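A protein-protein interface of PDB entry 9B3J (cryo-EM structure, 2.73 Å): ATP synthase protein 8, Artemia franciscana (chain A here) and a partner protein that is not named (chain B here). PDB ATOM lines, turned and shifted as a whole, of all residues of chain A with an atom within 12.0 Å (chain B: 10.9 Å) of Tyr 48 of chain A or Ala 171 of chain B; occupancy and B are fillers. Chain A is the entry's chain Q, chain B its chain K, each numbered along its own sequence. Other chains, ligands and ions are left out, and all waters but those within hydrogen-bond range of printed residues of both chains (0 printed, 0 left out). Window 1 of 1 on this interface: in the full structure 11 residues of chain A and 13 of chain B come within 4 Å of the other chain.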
ATOM      1  N   GLY A  41       4.786 -19.130  10.743  1.00  0.00           N
ATOM      2  CA  GLY A  41       3.645 -19.759  10.096  1.00  0.00           C
ATOM      3  C   GLY A  41       3.548 -19.440   8.618  1.00  0.00           C
ATOM      4  O   GLY A  41       3.104 -20.278   7.826  1.00  0.00           O
ATOM      5  N   PHE A  42       3.993 -18.244   8.221  1.00  0.00           N
ATOM      6  CA  PHE A  42       4.008 -17.866   6.813  1.00  0.00           C
ATOM      7  C   PHE A  42       4.996 -18.687   5.997  1.00  0.00           C
ATOM      8  O   PHE A  42       4.916 -18.674   4.763  1.00  0.00           O
ATOM      9  CB  PHE A  42       4.331 -16.381   6.668  1.00  0.00           C
ATOM     10  CG  PHE A  42       3.199 -15.477   7.054  1.00  0.00           C
ATOM     11  CD1 PHE A  42       2.248 -15.102   6.120  1.00  0.00           C
ATOM     12  CD2 PHE A  42       3.088 -14.997   8.349  1.00  0.00           C
ATOM     13  CE1 PHE A  42       1.204 -14.270   6.469  1.00  0.00           C
ATOM     14  CE2 PHE A  42       2.045 -14.164   8.705  1.00  0.00           C
ATOM     15  CZ  PHE A  42       1.103 -13.799   7.763  1.00  0.00           C
ATOM     16  N   SER A  43       5.923 -19.398   6.649  1.00  0.00           N
ATOM     17  CA  SER A  43       6.783 -20.323   5.921  1.00  0.00           C
ATOM     18  C   SER A  43       6.035 -21.559   5.441  1.00  0.00           C
ATOM     19  O   SER A  43       6.572 -22.301   4.611  1.00  0.00           O
ATOM     20  CB  SER A  43       7.959 -20.747   6.797  1.00  0.00           C
ATOM     21  OG  SER A  43       7.510 -21.505   7.907  1.00  0.00           O
ATOM     22  N   ASP A  44       4.822 -21.805   5.945  1.00  0.00           N
ATOM     23  CA  ASP A  44       4.016 -22.923   5.481  1.00  0.00           C
ATOM     24  C   ASP A  44       2.614 -22.521   5.049  1.00  0.00           C
ATOM     25  O   ASP A  44       1.824 -23.398   4.686  1.00  0.00           O
ATOM     26  CB  ASP A  44       3.916 -24.004   6.569  1.00  0.00           C
ATOM     27  CG  ASP A  44       5.236 -24.707   6.815  1.00  0.00           C
ATOM     28  OD1 ASP A  44       5.996 -24.898   5.845  1.00  0.00           O
ATOM     29  OD2 ASP A  44       5.513 -25.068   7.978  1.00  0.00           O
ATOM     30  N   ARG A  45       2.277 -21.230   5.083  1.00  0.00           N
ATOM     31  CA  ARG A  45       0.940 -20.813   4.673  1.00  0.00           C
ATOM     32  C   ARG A  45       0.762 -20.886   3.163  1.00  0.00           C
ATOM     33  O   ARG A  45      -0.340 -21.181   2.688  1.00  0.00           O
ATOM     34  CB  ARG A  45       0.646 -19.396   5.168  1.00  0.00           C
ATOM     35  CG  ARG A  45       0.213 -19.320   6.623  1.00  0.00           C
ATOM     36  CD  ARG A  45      -0.279 -17.929   6.979  1.00  0.00           C
ATOM     37  NE  ARG A  45      -0.684 -17.836   8.377  1.00  0.00           N
ATOM     38  CZ  ARG A  45      -1.273 -16.778   8.920  1.00  0.00           C
ATOM     39  NH1 ARG A  45      -1.558 -15.702   8.204  1.00  0.00           N
ATOM     40  NH2 ARG A  45      -1.586 -16.801  10.212  1.00  0.00           N
ATOM     41  N   THR A  46       1.818 -20.622   2.397  1.00  0.00           N
ATOM     42  CA  THR A  46       1.698 -20.625   0.945  1.00  0.00           C
ATOM     43  C   THR A  46       1.600 -22.053   0.431  1.00  0.00           C
ATOM     44  O   THR A  46       2.400 -22.918   0.798  1.00  0.00           O
ATOM     45  CB  THR A  46       2.888 -19.916   0.300  1.00  0.00           C
ATOM     46  OG1 THR A  46       4.042 -20.761   0.364  1.00  0.00           O
ATOM     47  CG2 THR A  46       3.182 -18.610   1.019  1.00  0.00           C
ATOM     48  N   VAL A  47       0.608 -22.296  -0.419  1.00  0.00           N
ATOM     49  CA  VAL A  47       0.364 -23.603  -1.014  1.00  0.00           C
ATOM     50  C   VAL A  47       0.500 -23.459  -2.522  1.00  0.00           C
ATOM     51  O   VAL A  47      -0.076 -22.538  -3.114  1.00  0.00           O
ATOM     52  CB  VAL A  47      -1.023 -24.152  -0.633  1.00  0.00           C
ATOM     53  CG1 VAL A  47      -1.234 -25.536  -1.225  1.00  0.00           C
ATOM     54  CG2 VAL A  47      -1.184 -24.187   0.878  1.00  0.00           C
ATOM     55  N   TYR A  48       1.268 -24.354  -3.134  1.00  0.00           N
ATOM     56  CA  TYR A  48       1.480 -24.306  -4.569  1.00  0.00           C
ATOM     57  C   TYR A  48       0.199 -24.664  -5.315  1.00  0.00           C
ATOM     58  O   TYR A  48      -0.726 -25.270  -4.767  1.00  0.00           O
ATOM     59  CB  TYR A  48       2.599 -25.262  -4.979  1.00  0.00           C
ATOM     60  CG  TYR A  48       3.819 -25.209  -4.090  1.00  0.00           C
ATOM     61  CD1 TYR A  48       4.798 -24.243  -4.277  1.00  0.00           C
ATOM     62  CD2 TYR A  48       3.999 -26.139  -3.071  1.00  0.00           C
ATOM     63  CE1 TYR A  48       5.918 -24.198  -3.470  1.00  0.00           C
ATOM     64  CE2 TYR A  48       5.115 -26.102  -2.258  1.00  0.00           C
ATOM     65  CZ  TYR A  48       6.070 -25.130  -2.463  1.00  0.00           C
ATOM     66  OH  TYR A  48       7.182 -25.093  -1.654  1.00  0.00           O
ATOM     67  N   LEU A  49       0.154 -24.274  -6.585  1.00  0.00           N
ATOM     68  CA  LEU A  49      -1.012 -24.547  -7.414  1.00  0.00           C
ATOM     69  C   LEU A  49      -1.092 -26.031  -7.747  1.00  0.00           C
ATOM     70  O   LEU A  49      -0.113 -26.633  -8.199  1.00  0.00           O
ATOM     71  CB  LEU A  49      -0.955 -23.720  -8.696  1.00  0.00           C
ATOM     72  CG  LEU A  49      -2.035 -24.005  -9.741  1.00  0.00           C
ATOM     73  CD1 LEU A  49      -3.425 -23.815  -9.155  1.00  0.00           C
ATOM     74  CD2 LEU A  49      -1.838 -23.112 -10.951  1.00  0.00           C
ATOM     75  N   ASN A  50      -2.266 -26.615  -7.532  1.00  0.00           N
ATOM     76  CA  ASN A  50      -2.475 -28.021  -7.834  1.00  0.00           C
ATOM     77  C   ASN A  50      -2.633 -28.223  -9.333  1.00  0.00           C
ATOM     78  O   ASN A  50      -3.288 -27.433 -10.018  1.00  0.00           O
ATOM     79  CB  ASN A  50      -3.705 -28.550  -7.101  1.00  0.00           C
ATOM     80  CG  ASN A  50      -3.568 -28.454  -5.599  1.00  0.00           C
ATOM     81  OD1 ASN A  50      -2.458 -28.407  -5.069  1.00  0.00           O
ATOM     82  ND2 ASN A  50      -4.696 -28.426  -4.901  1.00  0.00           N
ATOM     83  N   TRP A  51      -2.028 -29.289  -9.838  1.00  0.00           N
ATOM     84  CA  TRP A  51      -2.067 -29.598 -11.257  1.00  0.00           C
ATOM     85  C   TRP A  51      -3.297 -30.452 -11.543  1.00  0.00           C
ATOM     86  O   TRP A  51      -4.189 -30.600 -10.702  1.00  0.00           O
ATOM     87  CB  TRP A  51      -0.787 -30.306 -11.696  1.00  0.00           C
ATOM     88  CG  TRP A  51       0.480 -29.512 -11.543  1.00  0.00           C
ATOM     89  CD1 TRP A  51       0.630 -28.286 -10.959  1.00  0.00           C
ATOM     90  CD2 TRP A  51       1.781 -29.899 -11.994  1.00  0.00           C
ATOM     91  NE1 TRP A  51       1.943 -27.893 -11.013  1.00  0.00           N
ATOM     92  CE2 TRP A  51       2.670 -28.866 -11.645  1.00  0.00           C
ATOM     93  CE3 TRP A  51       2.282 -31.022 -12.657  1.00  0.00           C
ATOM     94  CZ2 TRP A  51       4.029 -28.925 -11.937  1.00  0.00           C
ATOM     95  CZ3 TRP A  51       3.628 -31.077 -12.947  1.00  0.00           C
ATOM     96  CH2 TRP A  51       4.487 -30.037 -12.588  1.00  0.00           C
ATOM     97  N   LYS A  52      -3.358 -31.029 -12.738  1.00  0.00           N
ATOM     98  CA  LYS A  52      -4.424 -31.946 -13.106  1.00  0.00           C
ATOM     99  C   LYS A  52      -3.821 -33.307 -13.420  1.00  0.00           C
ATOM    100  O   LYS A  52      -2.902 -33.412 -14.237  1.00  0.00           O
ATOM    101  CB  LYS A  52      -5.222 -31.417 -14.298  1.00  0.00           C
ATOM    102  CG  LYS A  52      -6.000 -30.145 -13.988  1.00  0.00           C
ATOM    103  CD  LYS A  52      -6.984 -29.815 -15.095  1.00  0.00           C
ATOM    104  CE  LYS A  52      -7.882 -28.649 -14.712  1.00  0.00           C
ATOM    105  NZ  LYS A  52      -8.932 -28.411 -15.740  1.00  0.00           N
ATOM    106  N   TRP A  53      -4.333 -34.337 -12.756  1.00  0.00           N
ATOM    107  CA  TRP A  53      -3.879 -35.704 -12.957  1.00  0.00           C
ATOM    108  C   TRP A  53      -5.082 -36.560 -13.259  1.00  0.00           C
ATOM    109  O   TRP A  53      -5.046 -37.791 -13.298  1.00  0.00           O
ATOM    110  CB  TRP A  53      -3.157 -36.224 -11.724  1.00  0.00           C
ATOM    111  CG  TRP A  53      -2.056 -35.340 -11.306  1.00  0.00           C
ATOM    112  CD1 TRP A  53      -2.114 -34.346 -10.380  1.00  0.00           C
ATOM    113  CD2 TRP A  53      -0.720 -35.346 -11.810  1.00  0.00           C
ATOM    114  NE1 TRP A  53      -0.890 -33.737 -10.266  1.00  0.00           N
ATOM    115  CE2 TRP A  53      -0.016 -34.336 -11.135  1.00  0.00           C
ATOM    116  CE3 TRP A  53      -0.048 -36.117 -12.762  1.00  0.00           C
ATOM    117  CZ2 TRP A  53       1.325 -34.074 -11.379  1.00  0.00           C
ATOM    118  CZ3 TRP A  53       1.283 -35.854 -13.005  1.00  0.00           C
ATOM    119  CH2 TRP A  53       1.955 -34.840 -12.318  1.00  0.00           C
ATOM    120  OXT TRP A  53      -6.136 -35.970 -13.442  1.00  0.00           O
ATOM    121  N   GLU B 163      11.340 -15.690   2.854  1.00  0.00           N
ATOM    122  CA  GLU B 163      11.008 -17.072   2.526  1.00  0.00           C
ATOM    123  C   GLU B 163       9.638 -17.175   1.872  1.00  0.00           C
ATOM    124  O   GLU B 163       9.436 -18.002   0.973  1.00  0.00           O
ATOM    125  CB  GLU B 163      11.060 -17.944   3.778  1.00  0.00           C
ATOM    126  CG  GLU B 163      12.455 -18.251   4.273  1.00  0.00           C
ATOM    127  CD  GLU B 163      12.442 -19.151   5.490  1.00  0.00           C
ATOM    128  OE1 GLU B 163      11.344 -19.593   5.889  1.00  0.00           O
ATOM    129  OE2 GLU B 163      13.526 -19.415   6.049  1.00  0.00           O
ATOM    130  N   ALA B 164       8.682 -16.350   2.314  1.00  0.00           N
ATOM    131  CA  ALA B 164       7.364 -16.344   1.686  1.00  0.00           C
ATOM    132  C   ALA B 164       7.439 -15.866   0.240  1.00  0.00           C
ATOM    133  O   ALA B 164       6.726 -16.383  -0.633  1.00  0.00           O
ATOM    134  CB  ALA B 164       6.409 -15.472   2.494  1.00  0.00           C
ATOM    135  N   ILE B 165       8.305 -14.885  -0.031  1.00  0.00           N
ATOM    136  CA  ILE B 165       8.487 -14.414  -1.404  1.00  0.00           C
ATOM    137  C   ILE B 165       9.069 -15.520  -2.285  1.00  0.00           C
ATOM    138  O   ILE B 165       8.594 -15.767  -3.407  1.00  0.00           O
ATOM    139  CB  ILE B 165       9.363 -13.152  -1.416  1.00  0.00           C
ATOM    140  CG1 ILE B 165       8.597 -11.988  -0.797  1.00  0.00           C
ATOM    141  CG2 ILE B 165       9.796 -12.799  -2.827  1.00  0.00           C
ATOM    142  CD1 ILE B 165       7.303 -11.685  -1.508  1.00  0.00           C
ATOM    143  N   THR B 166      10.094 -16.216  -1.781  1.00  0.00           N
ATOM    144  CA  THR B 166      10.696 -17.302  -2.554  1.00  0.00           C
ATOM    145  C   THR B 166       9.727 -18.458  -2.771  1.00  0.00           C
ATOM    146  O   THR B 166       9.771 -19.121  -3.815  1.00  0.00           O
ATOM    147  CB  THR B 166      11.954 -17.814  -1.862  1.00  0.00           C
ATOM    148  OG1 THR B 166      11.611 -18.292  -0.555  1.00  0.00           O
ATOM    149  CG2 THR B 166      12.980 -16.703  -1.744  1.00  0.00           C
ATOM    150  N   LEU B 167       8.846 -18.713  -1.803  1.00  0.00           N
ATOM    151  CA  LEU B 167       7.856 -19.768  -1.977  1.00  0.00           C
ATOM    152  C   LEU B 167       6.815 -19.391  -3.022  1.00  0.00           C
ATOM    153  O   LEU B 167       6.329 -20.263  -3.755  1.00  0.00           O
ATOM    154  CB  LEU B 167       7.188 -20.086  -0.643  1.00  0.00           C
ATOM    155  CG  LEU B 167       7.730 -21.307   0.104  1.00  0.00           C
ATOM    156  CD1 LEU B 167       9.247 -21.271   0.241  1.00  0.00           C
ATOM    157  CD2 LEU B 167       7.082 -21.407   1.468  1.00  0.00           C
ATOM    158  N   GLU B 168       6.466 -18.102  -3.110  1.00  0.00           N
ATOM    159  CA  GLU B 168       5.589 -17.661  -4.195  1.00  0.00           C
ATOM    160  C   GLU B 168       6.260 -17.826  -5.554  1.00  0.00           C
ATOM    161  O   GLU B 168       5.604 -18.194  -6.542  1.00  0.00           O
ATOM    162  CB  GLU B 168       5.171 -16.210  -3.976  1.00  0.00           C
ATOM    163  CG  GLU B 168       4.263 -16.009  -2.777  1.00  0.00           C
ATOM    164  CD  GLU B 168       2.919 -16.692  -2.934  1.00  0.00           C
ATOM    165  OE1 GLU B 168       2.416 -16.774  -4.073  1.00  0.00           O
ATOM    166  OE2 GLU B 168       2.362 -17.147  -1.914  1.00  0.00           O
ATOM    167  N   GLU B 169       7.567 -17.559  -5.620  1.00  0.00           N
ATOM    168  CA  GLU B 169       8.308 -17.791  -6.862  1.00  0.00           C
ATOM    169  C   GLU B 169       8.313 -19.270  -7.244  1.00  0.00           C
ATOM    170  O   GLU B 169       8.181 -19.620  -8.428  1.00  0.00           O
ATOM    171  CB  GLU B 169       9.736 -17.272  -6.717  1.00  0.00           C
ATOM    172  CG  GLU B 169       9.819 -15.796  -6.398  1.00  0.00           C
ATOM    173  CD  GLU B 169      11.138 -15.415  -5.757  1.00  0.00           C
ATOM    174  OE1 GLU B 169      11.982 -16.312  -5.551  1.00  0.00           O
ATOM    175  OE2 GLU B 169      11.333 -14.221  -5.454  1.00  0.00           O
ATOM    176  N   ARG B 170       8.468 -20.153  -6.252  1.00  0.00           N
ATOM    177  CA  ARG B 170       8.403 -21.589  -6.515  1.00  0.00           C
ATOM    178  C   ARG B 170       7.017 -22.008  -6.991  1.00  0.00           C
ATOM    179  O   ARG B 170       6.887 -22.909  -7.827  1.00  0.00           O
ATOM    180  CB  ARG B 170       8.789 -22.378  -5.268  1.00  0.00           C
ATOM    181  CG  ARG B 170      10.267 -22.371  -4.949  1.00  0.00           C
ATOM    182  CD  ARG B 170      10.594 -23.411  -3.890  1.00  0.00           C
ATOM    183  NE  ARG B 170      12.024 -23.480  -3.617  1.00  0.00           N
ATOM    184  CZ  ARG B 170      12.629 -22.859  -2.613  1.00  0.00           C
ATOM    185  NH1 ARG B 170      11.950 -22.128  -1.744  1.00  0.00           N
ATOM    186  NH2 ARG B 170      13.946 -22.976  -2.477  1.00  0.00           N
ATOM    187  N   ALA B 171       5.970 -21.374  -6.456  1.00  0.00           N
ATOM    188  CA  ALA B 171       4.611 -21.671  -6.908  1.00  0.00           C
ATOM    189  C   ALA B 171       4.404 -21.263  -8.363  1.00  0.00           C
ATOM    190  O   ALA B 171       3.738 -21.973  -9.132  1.00  0.00           O
ATOM    191  CB  ALA B 171       3.599 -20.970  -6.007  1.00  0.00           C
ATOM    192  N   GLN B 172       4.968 -20.119  -8.756  1.00  0.00           N
ATOM    193  CA  GLN B 172       4.890 -19.700 -10.155  1.00  0.00           C
ATOM    194  C   GLN B 172       5.637 -20.666 -11.073  1.00  0.00           C
ATOM    195  O   GLN B 172       5.157 -21.001 -12.170  1.00  0.00           O
ATOM    196  CB  GLN B 172       5.441 -18.285 -10.294  1.00  0.00           C
ATOM    197  CG  GLN B 172       4.649 -17.262  -9.506  1.00  0.00           C
ATOM    198  CD  GLN B 172       5.448 -16.017  -9.202  1.00  0.00           C
ATOM    199  OE1 GLN B 172       6.667 -15.990  -9.374  1.00  0.00           O
ATOM    200  NE2 GLN B 172       4.766 -14.974  -8.748  1.00  0.00           N
ATOM    201  N   LYS B 173       6.812 -21.131 -10.635  1.00  0.00           N
ATOM    202  CA  LYS B 173       7.539 -22.140 -11.404  1.00  0.00           C
ATOM    203  C   LYS B 173       6.776 -23.459 -11.473  1.00  0.00           C
ATOM    204  O   LYS B 173       6.866 -24.181 -12.477  1.00  0.00           O
ATOM    205  CB  LYS B 173       8.925 -22.359 -10.802  1.00  0.00           C
ATOM    206  CG  LYS B 173       9.802 -21.126 -10.834  1.00  0.00           C
ATOM    207  CD  LYS B 173      11.151 -21.392 -10.200  1.00  0.00           C
ATOM    208  CE  LYS B 173      11.965 -20.115 -10.084  1.00  0.00           C
ATOM    209  NZ  LYS B 173      11.279 -19.097  -9.240  1.00  0.00           N
ATOM    210  N   SER B 174       6.021 -23.788 -10.423  1.00  0.00           N
ATOM    211  CA  SER B 174       5.173 -24.974 -10.461  1.00  0.00           C
ATOM    212  C   SER B 174       4.063 -24.827 -11.494  1.00  0.00           C
ATOM    213  O   SER B 174       3.687 -25.803 -12.152  1.00  0.00           O
ATOM    214  CB  SER B 174       4.587 -25.246  -9.079  1.00  0.00           C
ATOM    215  OG  SER B 174       3.727 -26.371  -9.116  1.00  0.00           O
ATOM    216  N   ALA B 175       3.520 -23.615 -11.642  1.00  0.00           N
ATOM    217  CA  ALA B 175       2.516 -23.380 -12.682  1.00  0.00           C
ATOM    218  C   ALA B 175       3.105 -23.548 -14.083  1.00  0.00           C
ATOM    219  O   ALA B 175       2.462 -24.121 -14.985  1.00  0.00           O
ATOM    220  CB  ALA B 175       1.916 -21.985 -12.519  1.00  0.00           C
ATOM    221  N   GLU B 176       4.332 -23.058 -14.281  1.00  0.00           N
ATOM    222  CA  GLU B 176       5.002 -23.241 -15.571  1.00  0.00           C
ATOM    223  C   GLU B 176       5.243 -24.722 -15.873  1.00  0.00           C
ATOM    224  O   GLU B 176       5.031 -25.192 -17.006  1.00  0.00           O
ATOM    225  CB  GLU B 176       6.320 -22.472 -15.576  1.00  0.00           C
ATOM    226  CG  GLU B 176       6.160 -21.001 -15.259  1.00  0.00           C
ATOM    227  CD  GLU B 176       7.368 -20.424 -14.554  1.00  0.00           C
ATOM    228  OE1 GLU B 176       8.448 -21.049 -14.614  1.00  0.00           O
ATOM    229  OE2 GLU B 176       7.236 -19.350 -13.932  1.00  0.00           O
ATOM    230  N   ALA B 177       5.672 -25.480 -14.866  1.00  0.00           N
ATOM    231  CA  ALA B 177       5.862 -26.909 -15.069  1.00  0.00           C
ATOM    232  C   ALA B 177       4.542 -27.652 -15.230  1.00  0.00           C
ATOM    233  O   ALA B 177       4.525 -28.745 -15.804  1.00  0.00           O
ATOM    234  CB  ALA B 177       6.667 -27.497 -13.916  1.00  0.00           C
ATOM    235  N   GLN B 178       3.436 -27.083 -14.750  1.00  0.00           N
ATOM    236  CA  GLN B 178       2.128 -27.653 -15.060  1.00  0.00           C
ATOM    237  C   GLN B 178       1.812 -27.515 -16.546  1.00  0.00           C
ATOM    238  O   GLN B 178       1.210 -28.418 -17.153  1.00  0.00           O
ATOM    239  CB  GLN B 178       1.049 -26.978 -14.218  1.00  0.00           C
ATOM    240  CG  GLN B 178      -0.323 -27.593 -14.382  1.00  0.00           C
ATOM    241  CD  GLN B 178      -1.404 -26.785 -13.706  1.00  0.00           C
ATOM    242  OE1 GLN B 178      -2.548 -27.224 -13.600  1.00  0.00           O
ATOM    243  NE2 GLN B 178      -1.049 -25.591 -13.247  1.00  0.00           N
ATOM    244  N   ILE B 179       2.206 -26.386 -17.142  1.00  0.00           N
ATOM    245  CA  ILE B 179       2.069 -26.237 -18.596  1.00  0.00           C
ATOM    246  C   ILE B 179       2.896 -27.298 -19.322  1.00  0.00           C
ATOM    247  O   ILE B 179       2.453 -27.892 -20.325  1.00  0.00           O
ATOM    248  CB  ILE B 179       2.471 -24.817 -19.030  1.00  0.00           C
ATOM    249  CG1 ILE B 179       1.729 -23.780 -18.194  1.00  0.00           C
ATOM    250  CG2 ILE B 179       2.189 -24.605 -20.508  1.00  0.00           C
ATOM    251  CD1 ILE B 179       2.162 -22.362 -18.461  1.00  0.00           C
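Printed residues of chain B that touch a printed residue of chain A: Glu 163, Leu 167, Glu 168, Arg 170, Ala 171, Ser 174, Ala 177 and Gln 178.
Along chain B the printed residues that touch a printed residue of chain A span positions 163 to 178.
Of the 13 printed residues of chain A, 7 touch a printed residue of chain B.
Printed residues of chain A that touch a printed residue of chain B: Ser 43, Thr 46, Tyr 48, Leu 49, Asn 50, Trp 51 and Lys 52.
Among the printed residues, 14 pairs touch across the chains.
Among the printed residues, no Asp or Glu carboxylate lies within 4 Å of a Lys or Arg side-chain nitrogen of the other chain.
O of Glu 163 of chain B is in hydrogen-bond range of OG1 of Thr 166 of chain B (2.7 Å).
The indole nitrogen of Trp 51 of chain A lies within hydrogen-bond range of the backbone carbonyl oxygen of Ser 174 of chain B.
Among the printed residues, merely in contact across the chains: Thr 46 of chain A with Leu 167 of chain B (3.3 Å), Ser 43 of chain A with Leu 167 of chain B (3.3 Å), Trp 51 of chain A with Gln 178 of chain B (3.4 Å), Thr 46 of chain A with Glu 168 of chain B (3.4 Å), Trp 51 of chain A with Ala 177 of chain B (3.5 Å), Leu 49 of chain A with Gln 178 of chain B (3.5 Å), Asn 50 of chain A with Gln 178 of chain B (3.7 Å), Tyr 48 of chain A with Ala 171 of chain B (3.7 Å), Ser 43 of chain A with Glu 163 of chain B (3.7 Å), Tyr 48 of chain A with Arg 170 of chain B (3.8 Å), Leu 49 of chain A with Ser 174 of chain B (3.96 Å), Tyr 48 of chain A with Leu 167 of chain B (3.97 Å) and Lys 52 of chain A with Gln 178 of chain B (3.98 Å).
Printed residues of chain B within 4 Å of Thr 46 of chain A: Leu 167 and Glu 168.
No residue of chain B comes within 4 Å of Val 47 of chain A.
Of chain B, only Leu 167, Arg 170 and Ala 171 come within 4 Å of Tyr 48 of chain A.
Printed residues of chain B within 4 Å of Asn 50 of chain A: Gln 178 (3.7 Å).
Of the printed residues of chain B, Trp 51 of chain A touches Ser 174 (3.0 Å), Ala 177 (3.5 Å) and Gln 178 (3.4 Å).
Of the printed residues of chain B, Lys 52 of chain A touches Gln 178 (3.98 Å).
Printed residues of chain A within 4 Å of Glu 163 of chain B: Ser 43 (3.7 Å).
Leu 167 of chain B touches just these residues of chain A: Ser 43, Thr 46 and Tyr 48.
Glu 168 of chain B touches just one residue of chain A: Thr 46 (3.4 Å).
Of chain A, only Tyr 48 comes within 4 Å of Arg 170 of chain B.
Of chain A, only Tyr 48 (3.7 Å) comes within 4 Å of Ala 171 of chain B.
No residue of chain A comes within 4 Å of Gln 172 of chain B.
No residue of chain A comes within 4 Å of Lys 173 of chain B.
Of the printed residues of chain A, Ser 174 of chain B touches Leu 49 and Trp 51.
No residue of chain A comes within 4 Å of Ala 175 of chain B.
The nearest residue of chain B that does not touch Tyr 48 of chain A is Ser 174 of chain B (4.4 Å).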
